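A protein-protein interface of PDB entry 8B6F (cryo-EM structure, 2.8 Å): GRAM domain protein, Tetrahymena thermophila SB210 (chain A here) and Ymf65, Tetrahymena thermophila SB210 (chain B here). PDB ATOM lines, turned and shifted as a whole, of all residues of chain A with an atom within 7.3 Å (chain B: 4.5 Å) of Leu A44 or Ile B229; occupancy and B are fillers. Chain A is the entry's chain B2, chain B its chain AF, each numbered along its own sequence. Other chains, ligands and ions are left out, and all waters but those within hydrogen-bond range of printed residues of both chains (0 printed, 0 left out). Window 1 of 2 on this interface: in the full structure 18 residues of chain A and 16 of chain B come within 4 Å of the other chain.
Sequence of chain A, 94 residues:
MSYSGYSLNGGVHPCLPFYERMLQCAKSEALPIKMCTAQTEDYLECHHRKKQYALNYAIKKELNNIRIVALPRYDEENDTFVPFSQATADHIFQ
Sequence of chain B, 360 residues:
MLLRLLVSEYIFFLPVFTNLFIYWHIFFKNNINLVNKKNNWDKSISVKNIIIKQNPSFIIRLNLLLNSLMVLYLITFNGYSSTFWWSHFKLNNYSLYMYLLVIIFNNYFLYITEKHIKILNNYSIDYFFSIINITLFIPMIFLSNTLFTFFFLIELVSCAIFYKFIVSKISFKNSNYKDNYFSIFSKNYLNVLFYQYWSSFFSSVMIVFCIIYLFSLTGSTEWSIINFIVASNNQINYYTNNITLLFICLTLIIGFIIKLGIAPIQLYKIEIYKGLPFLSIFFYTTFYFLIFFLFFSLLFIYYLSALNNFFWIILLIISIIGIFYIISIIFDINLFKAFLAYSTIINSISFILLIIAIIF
OH of Tyr B238 sits at hydrogen-bond distance from OE1 of Glu A45, 2.7 Å away. O of Tyr B238 sits at hydrogen-bond distance from NZ of Lys A50. The side-chain hydroxyl of Tyr B238 lies within hydrogen-bond range of the backbone carbonyl oxygen of Leu A44 (3.4 Å).
Printed residues of chain A that touch a printed residue of chain B: Tyr A19, Met A22, Ile A33, Thr A40, Tyr A43, Leu A44, Glu A45, His A48, Arg A49 and Lys A50. Hydrophobic or aromatic side chains of chain A within 4 Å of the printed part of chain B: Tyr A19, Met A22, Ile A33, Tyr A43, Leu A44 and His A48. Of the 11 printed residues of chain B, 6 touch a printed residue of chain A. Hydrophobic or aromatic side chains of chain B that line the printed part of chain A: Ile B225, Phe B228, Ile B229, Ala B231 and Tyr B238. Among the printed residues, no Asp or Glu carboxylate lies within 4 Å of a Lys or Arg side-chain nitrogen of the other chain.
The backbone carbonyl oxygen (O) of His A47 is in hydrogen-bond range of the guanidinium group (NH2) of Arg A49 (3.4 Å). The backbone carbonyl oxygen (O) of Phe B228 lies within hydrogen-bond range of the side-chain hydroxyl (OG) of Ser B232 (3.0 Å).
Leu A44 touches two residues of chain B. Of the printed residues of chain A, Ala B231 touches Ile A33 (3.4 Å). Printed residues of chain A within 4 Å of Ser B232: Thr A40 (3.3 Å). Of the printed residues of chain A, Ile B225 touches Tyr A19. Of the printed residues of chain B, Tyr A43 touches Ile B229 (3.7 Å). Printed residues of chain B within 4 Å of Met A22: Phe B228 (3.5 Å) and Ile B229 (3.6 Å). Ile B226 touches none of the printed residues of chain A. The nearest printed residue of chain B that does not touch Leu A44 is Asn B233 (4.6 Å).
Tyr A19 touches Ile B225. Met A22 touches Phe B228. CD1 of Phe B228 touches CD1 of Ile A33, at 3.6 Å. Ala B231 touches Ile A33. Phe B228 touches Thr A40. CB of Ser B232 touches CG2 of Thr A40, 3.3 Å away. Tyr A43 touches Ile B229. Leu A44 touches Ile B229. CB of His A48 touches OH of Tyr B238 (3.7 Å). Arg A49 touches Tyr B238.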
ATOM      1  N   CYS A  15     -20.436  23.731  -1.507  1.00  0.00           N
ATOM      2  CA  CYS A  15     -19.965  23.776  -2.886  1.00  0.00           C
ATOM      3  C   CYS A  15     -19.846  22.398  -3.521  1.00  0.00           C
ATOM      4  O   CYS A  15     -19.481  22.308  -4.697  1.00  0.00           O
ATOM      5  CB  CYS A  15     -18.606  24.481  -2.961  1.00  0.00           C
ATOM      6  SG  CYS A  15     -18.613  26.178  -2.359  1.00  0.00           S
ATOM      7  N   PHE A  18     -21.545  21.777  -7.045  1.00  0.00           N
ATOM      8  CA  PHE A  18     -20.868  22.501  -8.116  1.00  0.00           C
ATOM      9  C   PHE A  18     -19.495  21.908  -8.397  1.00  0.00           C
ATOM     10  O   PHE A  18     -19.088  21.784  -9.557  1.00  0.00           O
ATOM     11  CB  PHE A  18     -20.743  23.979  -7.757  1.00  0.00           C
ATOM     12  CG  PHE A  18     -22.059  24.663  -7.553  1.00  0.00           C
ATOM     13  CD1 PHE A  18     -22.837  25.032  -8.634  1.00  0.00           C
ATOM     14  CD2 PHE A  18     -22.513  24.949  -6.279  1.00  0.00           C
ATOM     15  CE1 PHE A  18     -24.048  25.665  -8.449  1.00  0.00           C
ATOM     16  CE2 PHE A  18     -23.720  25.582  -6.086  1.00  0.00           C
ATOM     17  CZ  PHE A  18     -24.489  25.940  -7.174  1.00  0.00           C
ATOM     18  N   TYR A  19     -18.763  21.538  -7.344  1.00  0.00           N
ATOM     19  CA  TYR A  19     -17.442  20.948  -7.528  1.00  0.00           C
ATOM     20  C   TYR A  19     -17.533  19.625  -8.277  1.00  0.00           C
ATOM     21  O   TYR A  19     -16.732  19.358  -9.180  1.00  0.00           O
ATOM     22  CB  TYR A  19     -16.770  20.755  -6.170  1.00  0.00           C
ATOM     23  CG  TYR A  19     -15.377  20.178  -6.242  1.00  0.00           C
ATOM     24  CD1 TYR A  19     -14.271  21.002  -6.400  1.00  0.00           C
ATOM     25  CD2 TYR A  19     -15.166  18.812  -6.136  1.00  0.00           C
ATOM     26  CE1 TYR A  19     -12.995  20.479  -6.458  1.00  0.00           C
ATOM     27  CE2 TYR A  19     -13.896  18.279  -6.193  1.00  0.00           C
ATOM     28  CZ  TYR A  19     -12.815  19.117  -6.353  1.00  0.00           C
ATOM     29  OH  TYR A  19     -11.547  18.588  -6.410  1.00  0.00           O
ATOM     30  N   MET A  22     -18.271  20.362 -11.936  1.00  0.00           N
ATOM     31  CA  MET A  22     -17.090  20.874 -12.622  1.00  0.00           C
ATOM     32  C   MET A  22     -16.099  19.758 -12.918  1.00  0.00           C
ATOM     33  O   MET A  22     -15.552  19.677 -14.024  1.00  0.00           O
ATOM     34  CB  MET A  22     -16.430  21.956 -11.770  1.00  0.00           C
ATOM     35  CG  MET A  22     -15.181  22.564 -12.384  1.00  0.00           C
ATOM     36  SD  MET A  22     -14.369  23.741 -11.288  1.00  0.00           S
ATOM     37  CE  MET A  22     -13.873  22.674  -9.937  1.00  0.00           C
ATOM     38  N   ILE A  33     -11.070  23.417 -20.504  1.00  0.00           N
ATOM     39  CA  ILE A  33     -10.925  24.821 -20.127  1.00  0.00           C
ATOM     40  C   ILE A  33     -12.004  25.667 -20.785  1.00  0.00           C
ATOM     41  O   ILE A  33     -12.595  26.549 -20.150  1.00  0.00           O
ATOM     42  CB  ILE A  33      -9.514  25.328 -20.477  1.00  0.00           C
ATOM     43  CG1 ILE A  33      -8.457  24.590 -19.650  1.00  0.00           C
ATOM     44  CG2 ILE A  33      -9.405  26.836 -20.256  1.00  0.00           C
ATOM     45  CD1 ILE A  33      -8.649  24.688 -18.152  1.00  0.00           C
ATOM     46  N   THR A  37     -16.832  26.183 -18.914  1.00  0.00           N
ATOM     47  CA  THR A  37     -16.889  27.527 -18.354  1.00  0.00           C
ATOM     48  C   THR A  37     -18.086  27.689 -17.426  1.00  0.00           C
ATOM     49  O   THR A  37     -17.969  28.286 -16.350  1.00  0.00           O
ATOM     50  CB  THR A  37     -16.941  28.558 -19.481  1.00  0.00           C
ATOM     51  OG1 THR A  37     -18.041  28.267 -20.351  1.00  0.00           O
ATOM     52  CG2 THR A  37     -15.651  28.538 -20.282  1.00  0.00           C
ATOM     53  N   ALA A  38     -19.248  27.170 -17.825  1.00  0.00           N
ATOM     54  CA  ALA A  38     -20.448  27.338 -17.013  1.00  0.00           C
ATOM     55  C   ALA A  38     -20.288  26.678 -15.649  1.00  0.00           C
ATOM     56  O   ALA A  38     -20.524  27.305 -14.611  1.00  0.00           O
ATOM     57  CB  ALA A  38     -21.661  26.764 -17.746  1.00  0.00           C
ATOM     58  N   GLN A  39     -19.884  25.405 -15.630  1.00  0.00           N
ATOM     59  CA  GLN A  39     -19.731  24.705 -14.359  1.00  0.00           C
ATOM     60  C   GLN A  39     -18.651  25.343 -13.500  1.00  0.00           C
ATOM     61  O   GLN A  39     -18.829  25.511 -12.289  1.00  0.00           O
ATOM     62  CB  GLN A  39     -19.413  23.229 -14.603  1.00  0.00           C
ATOM     63  CG  GLN A  39     -20.586  22.416 -15.123  1.00  0.00           C
ATOM     64  CD  GLN A  39     -20.841  22.613 -16.598  1.00  0.00           C
ATOM     65  OE1 GLN A  39     -19.976  23.079 -17.335  1.00  0.00           O
ATOM     66  NE2 GLN A  39     -22.042  22.261 -17.038  1.00  0.00           N
ATOM     67  N   THR A  40     -17.520  25.703 -14.106  1.00  0.00           N
ATOM     68  CA  THR A  40     -16.431  26.297 -13.340  1.00  0.00           C
ATOM     69  C   THR A  40     -16.836  27.644 -12.759  1.00  0.00           C
ATOM     70  O   THR A  40     -16.490  27.964 -11.616  1.00  0.00           O
ATOM     71  CB  THR A  40     -15.180  26.442 -14.197  1.00  0.00           C
ATOM     72  OG1 THR A  40     -14.888  25.198 -14.845  1.00  0.00           O
ATOM     73  CG2 THR A  40     -14.019  26.807 -13.303  1.00  0.00           C
ATOM     74  N   GLU A  41     -17.564  28.451 -13.531  1.00  0.00           N
ATOM     75  CA  GLU A  41     -18.023  29.736 -13.020  1.00  0.00           C
ATOM     76  C   GLU A  41     -19.027  29.546 -11.893  1.00  0.00           C
ATOM     77  O   GLU A  41     -19.018  30.302 -10.915  1.00  0.00           O
ATOM     78  CB  GLU A  41     -18.639  30.561 -14.149  1.00  0.00           C
ATOM     79  CG  GLU A  41     -18.978  31.983 -13.744  1.00  0.00           C
ATOM     80  CD  GLU A  41     -19.371  32.843 -14.926  1.00  0.00           C
ATOM     81  OE1 GLU A  41     -19.424  32.312 -16.054  1.00  0.00           O
ATOM     82  OE2 GLU A  41     -19.622  34.050 -14.728  1.00  0.00           O
ATOM     83  N   ASP A  42     -19.903  28.550 -12.009  1.00  0.00           N
ATOM     84  CA  ASP A  42     -20.837  28.277 -10.923  1.00  0.00           C
ATOM     85  C   ASP A  42     -20.093  27.877  -9.656  1.00  0.00           C
ATOM     86  O   ASP A  42     -20.436  28.331  -8.559  1.00  0.00           O
ATOM     87  CB  ASP A  42     -21.815  27.177 -11.333  1.00  0.00           C
ATOM     88  CG  ASP A  42     -22.744  27.612 -12.443  1.00  0.00           C
ATOM     89  OD1 ASP A  42     -23.084  28.811 -12.496  1.00  0.00           O
ATOM     90  OD2 ASP A  42     -23.137  26.755 -13.260  1.00  0.00           O
ATOM     91  N   TYR A  43     -19.074  27.026  -9.783  1.00  0.00           N
ATOM     92  CA  TYR A  43     -18.299  26.633  -8.612  1.00  0.00           C
ATOM     93  C   TYR A  43     -17.580  27.831  -8.008  1.00  0.00           C
ATOM     94  O   TYR A  43     -17.591  28.029  -6.788  1.00  0.00           O
ATOM     95  CB  TYR A  43     -17.299  25.539  -8.987  1.00  0.00           C
ATOM     96  CG  TYR A  43     -16.230  25.319  -7.942  1.00  0.00           C
ATOM     97  CD1 TYR A  43     -16.505  24.629  -6.771  1.00  0.00           C
ATOM     98  CD2 TYR A  43     -14.944  25.807  -8.129  1.00  0.00           C
ATOM     99  CE1 TYR A  43     -15.531  24.431  -5.816  1.00  0.00           C
ATOM    100  CE2 TYR A  43     -13.964  25.614  -7.180  1.00  0.00           C
ATOM    101  CZ  TYR A  43     -14.263  24.925  -6.027  1.00  0.00           C
ATOM    102  OH  TYR A  43     -13.287  24.731  -5.081  1.00  0.00           O
ATOM    103  N   LEU A  44     -16.944  28.647  -8.852  1.00  0.00           N
ATOM    104  CA  LEU A  44     -16.235  29.819  -8.349  1.00  0.00           C
ATOM    105  C   LEU A  44     -17.196  30.796  -7.690  1.00  0.00           C
ATOM    106  O   LEU A  44     -16.849  31.449  -6.700  1.00  0.00           O
ATOM    107  CB  LEU A  44     -15.468  30.503  -9.479  1.00  0.00           C
ATOM    108  CG  LEU A  44     -14.252  29.752 -10.021  1.00  0.00           C
ATOM    109  CD1 LEU A  44     -13.623  30.511 -11.175  1.00  0.00           C
ATOM    110  CD2 LEU A  44     -13.236  29.522  -8.919  1.00  0.00           C
ATOM    111  N   GLU A  45     -18.413  30.904  -8.220  1.00  0.00           N
ATOM    112  CA  GLU A  45     -19.404  31.776  -7.605  1.00  0.00           C
ATOM    113  C   GLU A  45     -19.821  31.246  -6.242  1.00  0.00           C
ATOM    114  O   GLU A  45     -19.875  31.999  -5.263  1.00  0.00           O
ATOM    115  CB  GLU A  45     -20.613  31.920  -8.529  1.00  0.00           C
ATOM    116  CG  GLU A  45     -21.748  32.744  -7.944  1.00  0.00           C
ATOM    117  CD  GLU A  45     -21.302  34.121  -7.505  1.00  0.00           C
ATOM    118  OE1 GLU A  45     -20.265  34.601  -8.007  1.00  0.00           O
ATOM    119  OE2 GLU A  45     -21.985  34.721  -6.652  1.00  0.00           O
ATOM    120  N   CYS A  46     -20.122  29.951  -6.154  1.00  0.00           N
ATOM    121  CA  CYS A  46     -20.482  29.382  -4.863  1.00  0.00           C
ATOM    122  C   CYS A  46     -19.343  29.481  -3.860  1.00  0.00           C
ATOM    123  O   CYS A  46     -19.593  29.465  -2.651  1.00  0.00           O
ATOM    124  CB  CYS A  46     -20.893  27.919  -5.034  1.00  0.00           C
ATOM    125  SG  CYS A  46     -21.686  27.202  -3.584  1.00  0.00           S
ATOM    126  N   HIS A  47     -18.100  29.586  -4.332  1.00  0.00           N
ATOM    127  CA  HIS A  47     -16.944  29.656  -3.447  1.00  0.00           C
ATOM    128  C   HIS A  47     -16.640  31.081  -2.996  1.00  0.00           C
ATOM    129  O   HIS A  47     -16.415  31.322  -1.808  1.00  0.00           O
ATOM    130  CB  HIS A  47     -15.721  29.054  -4.146  1.00  0.00           C
ATOM    131  CG  HIS A  47     -14.484  29.061  -3.306  1.00  0.00           C
ATOM    132  ND1 HIS A  47     -14.388  28.371  -2.116  1.00  0.00           N
ATOM    133  CD2 HIS A  47     -13.292  29.677  -3.479  1.00  0.00           C
ATOM    134  CE1 HIS A  47     -13.189  28.560  -1.596  1.00  0.00           C
ATOM    135  NE2 HIS A  47     -12.504  29.348  -2.403  1.00  0.00           N
ATOM    136  N   HIS A  48     -16.630  32.034  -3.929  1.00  0.00           N
ATOM    137  CA  HIS A  48     -16.210  33.401  -3.643  1.00  0.00           C
ATOM    138  C   HIS A  48     -17.370  34.345  -3.369  1.00  0.00           C
ATOM    139  O   HIS A  48     -17.232  35.260  -2.551  1.00  0.00           O
ATOM    140  CB  HIS A  48     -15.381  33.956  -4.806  1.00  0.00           C
ATOM    141  CG  HIS A  48     -14.015  33.359  -4.914  1.00  0.00           C
ATOM    142  ND1 HIS A  48     -13.014  33.625  -4.004  1.00  0.00           N
ATOM    143  CD2 HIS A  48     -13.477  32.518  -5.828  1.00  0.00           C
ATOM    144  CE1 HIS A  48     -11.922  32.968  -4.350  1.00  0.00           C
ATOM    145  NE2 HIS A  48     -12.176  32.289  -5.453  1.00  0.00           N
ATOM    146  N   ARG A  49     -18.501  34.162  -4.049  1.00  0.00           N
ATOM    147  CA  ARG A  49     -19.679  35.008  -3.872  1.00  0.00           C
ATOM    148  C   ARG A  49     -19.430  36.430  -4.364  1.00  0.00           C
ATOM    149  O   ARG A  49     -19.958  37.391  -3.803  1.00  0.00           O
ATOM    150  CB  ARG A  49     -20.146  35.019  -2.413  1.00  0.00           C
ATOM    151  CG  ARG A  49     -20.615  33.661  -1.920  1.00  0.00           C
ATOM    152  CD  ARG A  49     -20.330  33.465  -0.444  1.00  0.00           C
ATOM    153  NE  ARG A  49     -18.915  33.230  -0.186  1.00  0.00           N
ATOM    154  CZ  ARG A  49     -18.396  33.025   1.016  1.00  0.00           C
ATOM    155  NH1 ARG A  49     -19.150  33.023   2.102  1.00  0.00           N
ATOM    156  NH2 ARG A  49     -17.089  32.816   1.132  1.00  0.00           N
ATOM    157  N   LYS A  50     -18.634  36.571  -5.424  1.00  0.00           N
ATOM    158  CA  LYS A  50     -18.349  37.892  -5.975  1.00  0.00           C
ATOM    159  C   LYS A  50     -19.617  38.556  -6.497  1.00  0.00           C
ATOM    160  O   LYS A  50     -19.839  39.750  -6.271  1.00  0.00           O
ATOM    161  CB  LYS A  50     -17.307  37.779  -7.088  1.00  0.00           C
ATOM    162  CG  LYS A  50     -16.981  39.092  -7.789  1.00  0.00           C
ATOM    163  CD  LYS A  50     -16.115  38.849  -9.013  1.00  0.00           C
ATOM    164  CE  LYS A  50     -15.931  40.118  -9.826  1.00  0.00           C
ATOM    165  NZ  LYS A  50     -15.169  39.865 -11.080  1.00  0.00           N
ATOM    166  N   THR B 218      -8.754  29.011  -4.574  1.00  0.00           N
ATOM    167  CA  THR B 218      -9.356  27.777  -5.056  1.00  0.00           C
ATOM    168  C   THR B 218      -9.689  26.894  -3.864  1.00  0.00           C
ATOM    169  O   THR B 218      -8.871  26.735  -2.954  1.00  0.00           O
ATOM    170  CB  THR B 218      -8.415  27.030  -6.001  1.00  0.00           C
ATOM    171  OG1 THR B 218      -7.347  26.444  -5.248  1.00  0.00           O
ATOM    172  CG2 THR B 218      -7.803  27.989  -7.009  1.00  0.00           C
ATOM    173  N   ILE B 225      -6.255  20.829  -9.658  1.00  0.00           N
ATOM    174  CA  ILE B 225      -7.383  21.726  -9.437  1.00  0.00           C
ATOM    175  C   ILE B 225      -6.932  23.180  -9.500  1.00  0.00           C
ATOM    176  O   ILE B 225      -7.632  24.034 -10.053  1.00  0.00           O
ATOM    177  CB  ILE B 225      -8.077  21.402  -8.101  1.00  0.00           C
ATOM    178  CG1 ILE B 225      -8.642  19.978  -8.115  1.00  0.00           C
ATOM    179  CG2 ILE B 225      -9.189  22.410  -7.822  1.00  0.00           C
ATOM    180  CD1 ILE B 225      -9.699  19.722  -9.174  1.00  0.00           C
ATOM    181  N   ILE B 226      -5.766  23.490  -8.930  1.00  0.00           N
ATOM    182  CA  ILE B 226      -5.267  24.862  -8.976  1.00  0.00           C
ATOM    183  C   ILE B 226      -5.080  25.306 -10.421  1.00  0.00           C
ATOM    184  O   ILE B 226      -5.539  26.381 -10.822  1.00  0.00           O
ATOM    185  CB  ILE B 226      -3.955  24.984  -8.177  1.00  0.00           C
ATOM    186  CG1 ILE B 226      -4.236  24.907  -6.676  1.00  0.00           C
ATOM    187  CG2 ILE B 226      -3.229  26.289  -8.514  1.00  0.00           C
ATOM    188  CD1 ILE B 226      -2.985  24.783  -5.830  1.00  0.00           C
ATOM    189  N   ASN B 227      -4.408  24.484 -11.226  1.00  0.00           N
ATOM    190  CA  ASN B 227      -4.169  24.862 -12.613  1.00  0.00           C
ATOM    191  C   ASN B 227      -5.478  25.005 -13.376  1.00  0.00           C
ATOM    192  O   ASN B 227      -5.664  25.966 -14.131  1.00  0.00           O
ATOM    193  CB  ASN B 227      -3.266  23.833 -13.290  1.00  0.00           C
ATOM    194  CG  ASN B 227      -1.862  23.847 -12.739  1.00  0.00           C
ATOM    195  OD1 ASN B 227      -1.028  24.649 -13.153  1.00  0.00           O
ATOM    196  ND2 ASN B 227      -1.589  22.952 -11.801  1.00  0.00           N
ATOM    197  N   PHE B 228      -6.398  24.059 -13.193  1.00  0.00           N
ATOM    198  CA  PHE B 228      -7.666  24.122 -13.908  1.00  0.00           C
ATOM    199  C   PHE B 228      -8.455  25.367 -13.524  1.00  0.00           C
ATOM    200  O   PHE B 228      -9.029  26.039 -14.388  1.00  0.00           O
ATOM    201  CB  PHE B 228      -8.480  22.859 -13.626  1.00  0.00           C
ATOM    202  CG  PHE B 228      -9.829  22.848 -14.279  1.00  0.00           C
ATOM    203  CD1 PHE B 228      -9.963  22.535 -15.617  1.00  0.00           C
ATOM    204  CD2 PHE B 228     -10.966  23.140 -13.545  1.00  0.00           C
ATOM    205  CE1 PHE B 228     -11.205  22.523 -16.217  1.00  0.00           C
ATOM    206  CE2 PHE B 228     -12.209  23.128 -14.138  1.00  0.00           C
ATOM    207  CZ  PHE B 228     -12.329  22.818 -15.477  1.00  0.00           C
ATOM    208  N   ILE B 229      -8.496  25.691 -12.232  1.00  0.00           N
ATOM    209  CA  ILE B 229      -9.247  26.858 -11.785  1.00  0.00           C
ATOM    210  C   ILE B 229      -8.615  28.144 -12.306  1.00  0.00           C
ATOM    211  O   ILE B 229      -9.320  29.072 -12.716  1.00  0.00           O
ATOM    212  CB  ILE B 229      -9.359  26.865 -10.250  1.00  0.00           C
ATOM    213  CG1 ILE B 229     -10.225  25.701  -9.755  1.00  0.00           C
ATOM    214  CG2 ILE B 229      -9.929  28.192  -9.779  1.00  0.00           C
ATOM    215  CD1 ILE B 229     -11.691  25.793 -10.116  1.00  0.00           C
ATOM    216  N   VAL B 230      -7.283  28.227 -12.295  1.00  0.00           N
ATOM    217  CA  VAL B 230      -6.612  29.429 -12.785  1.00  0.00           C
ATOM    218  C   VAL B 230      -6.865  29.615 -14.275  1.00  0.00           C
ATOM    219  O   VAL B 230      -7.130  30.731 -14.738  1.00  0.00           O
ATOM    220  CB  VAL B 230      -5.105  29.367 -12.472  1.00  0.00           C
ATOM    221  CG1 VAL B 230      -4.354  30.487 -13.182  1.00  0.00           C
ATOM    222  CG2 VAL B 230      -4.870  29.458 -10.976  1.00  0.00           C
ATOM    223  N   ALA B 231      -6.776  28.538 -15.052  1.00  0.00           N
ATOM    224  CA  ALA B 231      -7.025  28.652 -16.484  1.00  0.00           C
ATOM    225  C   ALA B 231      -8.470  29.047 -16.762  1.00  0.00           C
ATOM    226  O   ALA B 231      -8.736  29.898 -17.618  1.00  0.00           O
ATOM    227  CB  ALA B 231      -6.677  27.334 -17.171  1.00  0.00           C
ATOM    228  N   SER B 232      -9.417  28.440 -16.048  1.00  0.00           N
ATOM    229  CA  SER B 232     -10.824  28.779 -16.235  1.00  0.00           C
ATOM    230  C   SER B 232     -11.119  30.201 -15.785  1.00  0.00           C
ATOM    231  O   SER B 232     -11.984  30.868 -16.362  1.00  0.00           O
ATOM    232  CB  SER B 232     -11.705  27.801 -15.475  1.00  0.00           C
ATOM    233  OG  SER B 232     -11.521  26.474 -15.935  1.00  0.00           O
ATOM    234  N   ASN B 233     -10.418  30.675 -14.756  1.00  0.00           N
ATOM    235  CA  ASN B 233     -10.562  32.064 -14.343  1.00  0.00           C
ATOM    236  C   ASN B 233     -10.053  33.003 -15.426  1.00  0.00           C
ATOM    237  O   ASN B 233     -10.662  34.044 -15.688  1.00  0.00           O
ATOM    238  CB  ASN B 233      -9.813  32.294 -13.032  1.00  0.00           C
ATOM    239  CG  ASN B 233      -9.835  33.738 -12.597  1.00  0.00           C
ATOM    240  OD1 ASN B 233     -10.767  34.477 -12.910  1.00  0.00           O
ATOM    241  ND2 ASN B 233      -8.801  34.154 -11.877  1.00  0.00           N
ATOM    242  N   TYR B 238     -13.651  35.943 -14.362  1.00  0.00           N
ATOM    243  CA  TYR B 238     -14.467  36.070 -13.159  1.00  0.00           C
ATOM    244  C   TYR B 238     -13.680  36.713 -12.023  1.00  0.00           C
ATOM    245  O   TYR B 238     -14.041  37.789 -11.533  1.00  0.00           O
ATOM    246  CB  TYR B 238     -14.989  34.692 -12.745  1.00  0.00           C
ATOM    247  CG  TYR B 238     -15.673  34.669 -11.399  1.00  0.00           C
ATOM    248  CD1 TYR B 238     -17.037  34.899 -11.290  1.00  0.00           C
ATOM    249  CD2 TYR B 238     -14.955  34.409 -10.239  1.00  0.00           C
ATOM    250  CE1 TYR B 238     -17.666  34.878 -10.064  1.00  0.00           C
ATOM    251  CE2 TYR B 238     -15.574  34.384  -9.009  1.00  0.00           C
ATOM    252  CZ  TYR B 238     -16.930  34.620  -8.928  1.00  0.00           C
ATOM    253  OH  TYR B 238     -17.557  34.599  -7.707  1.00  0.00           O
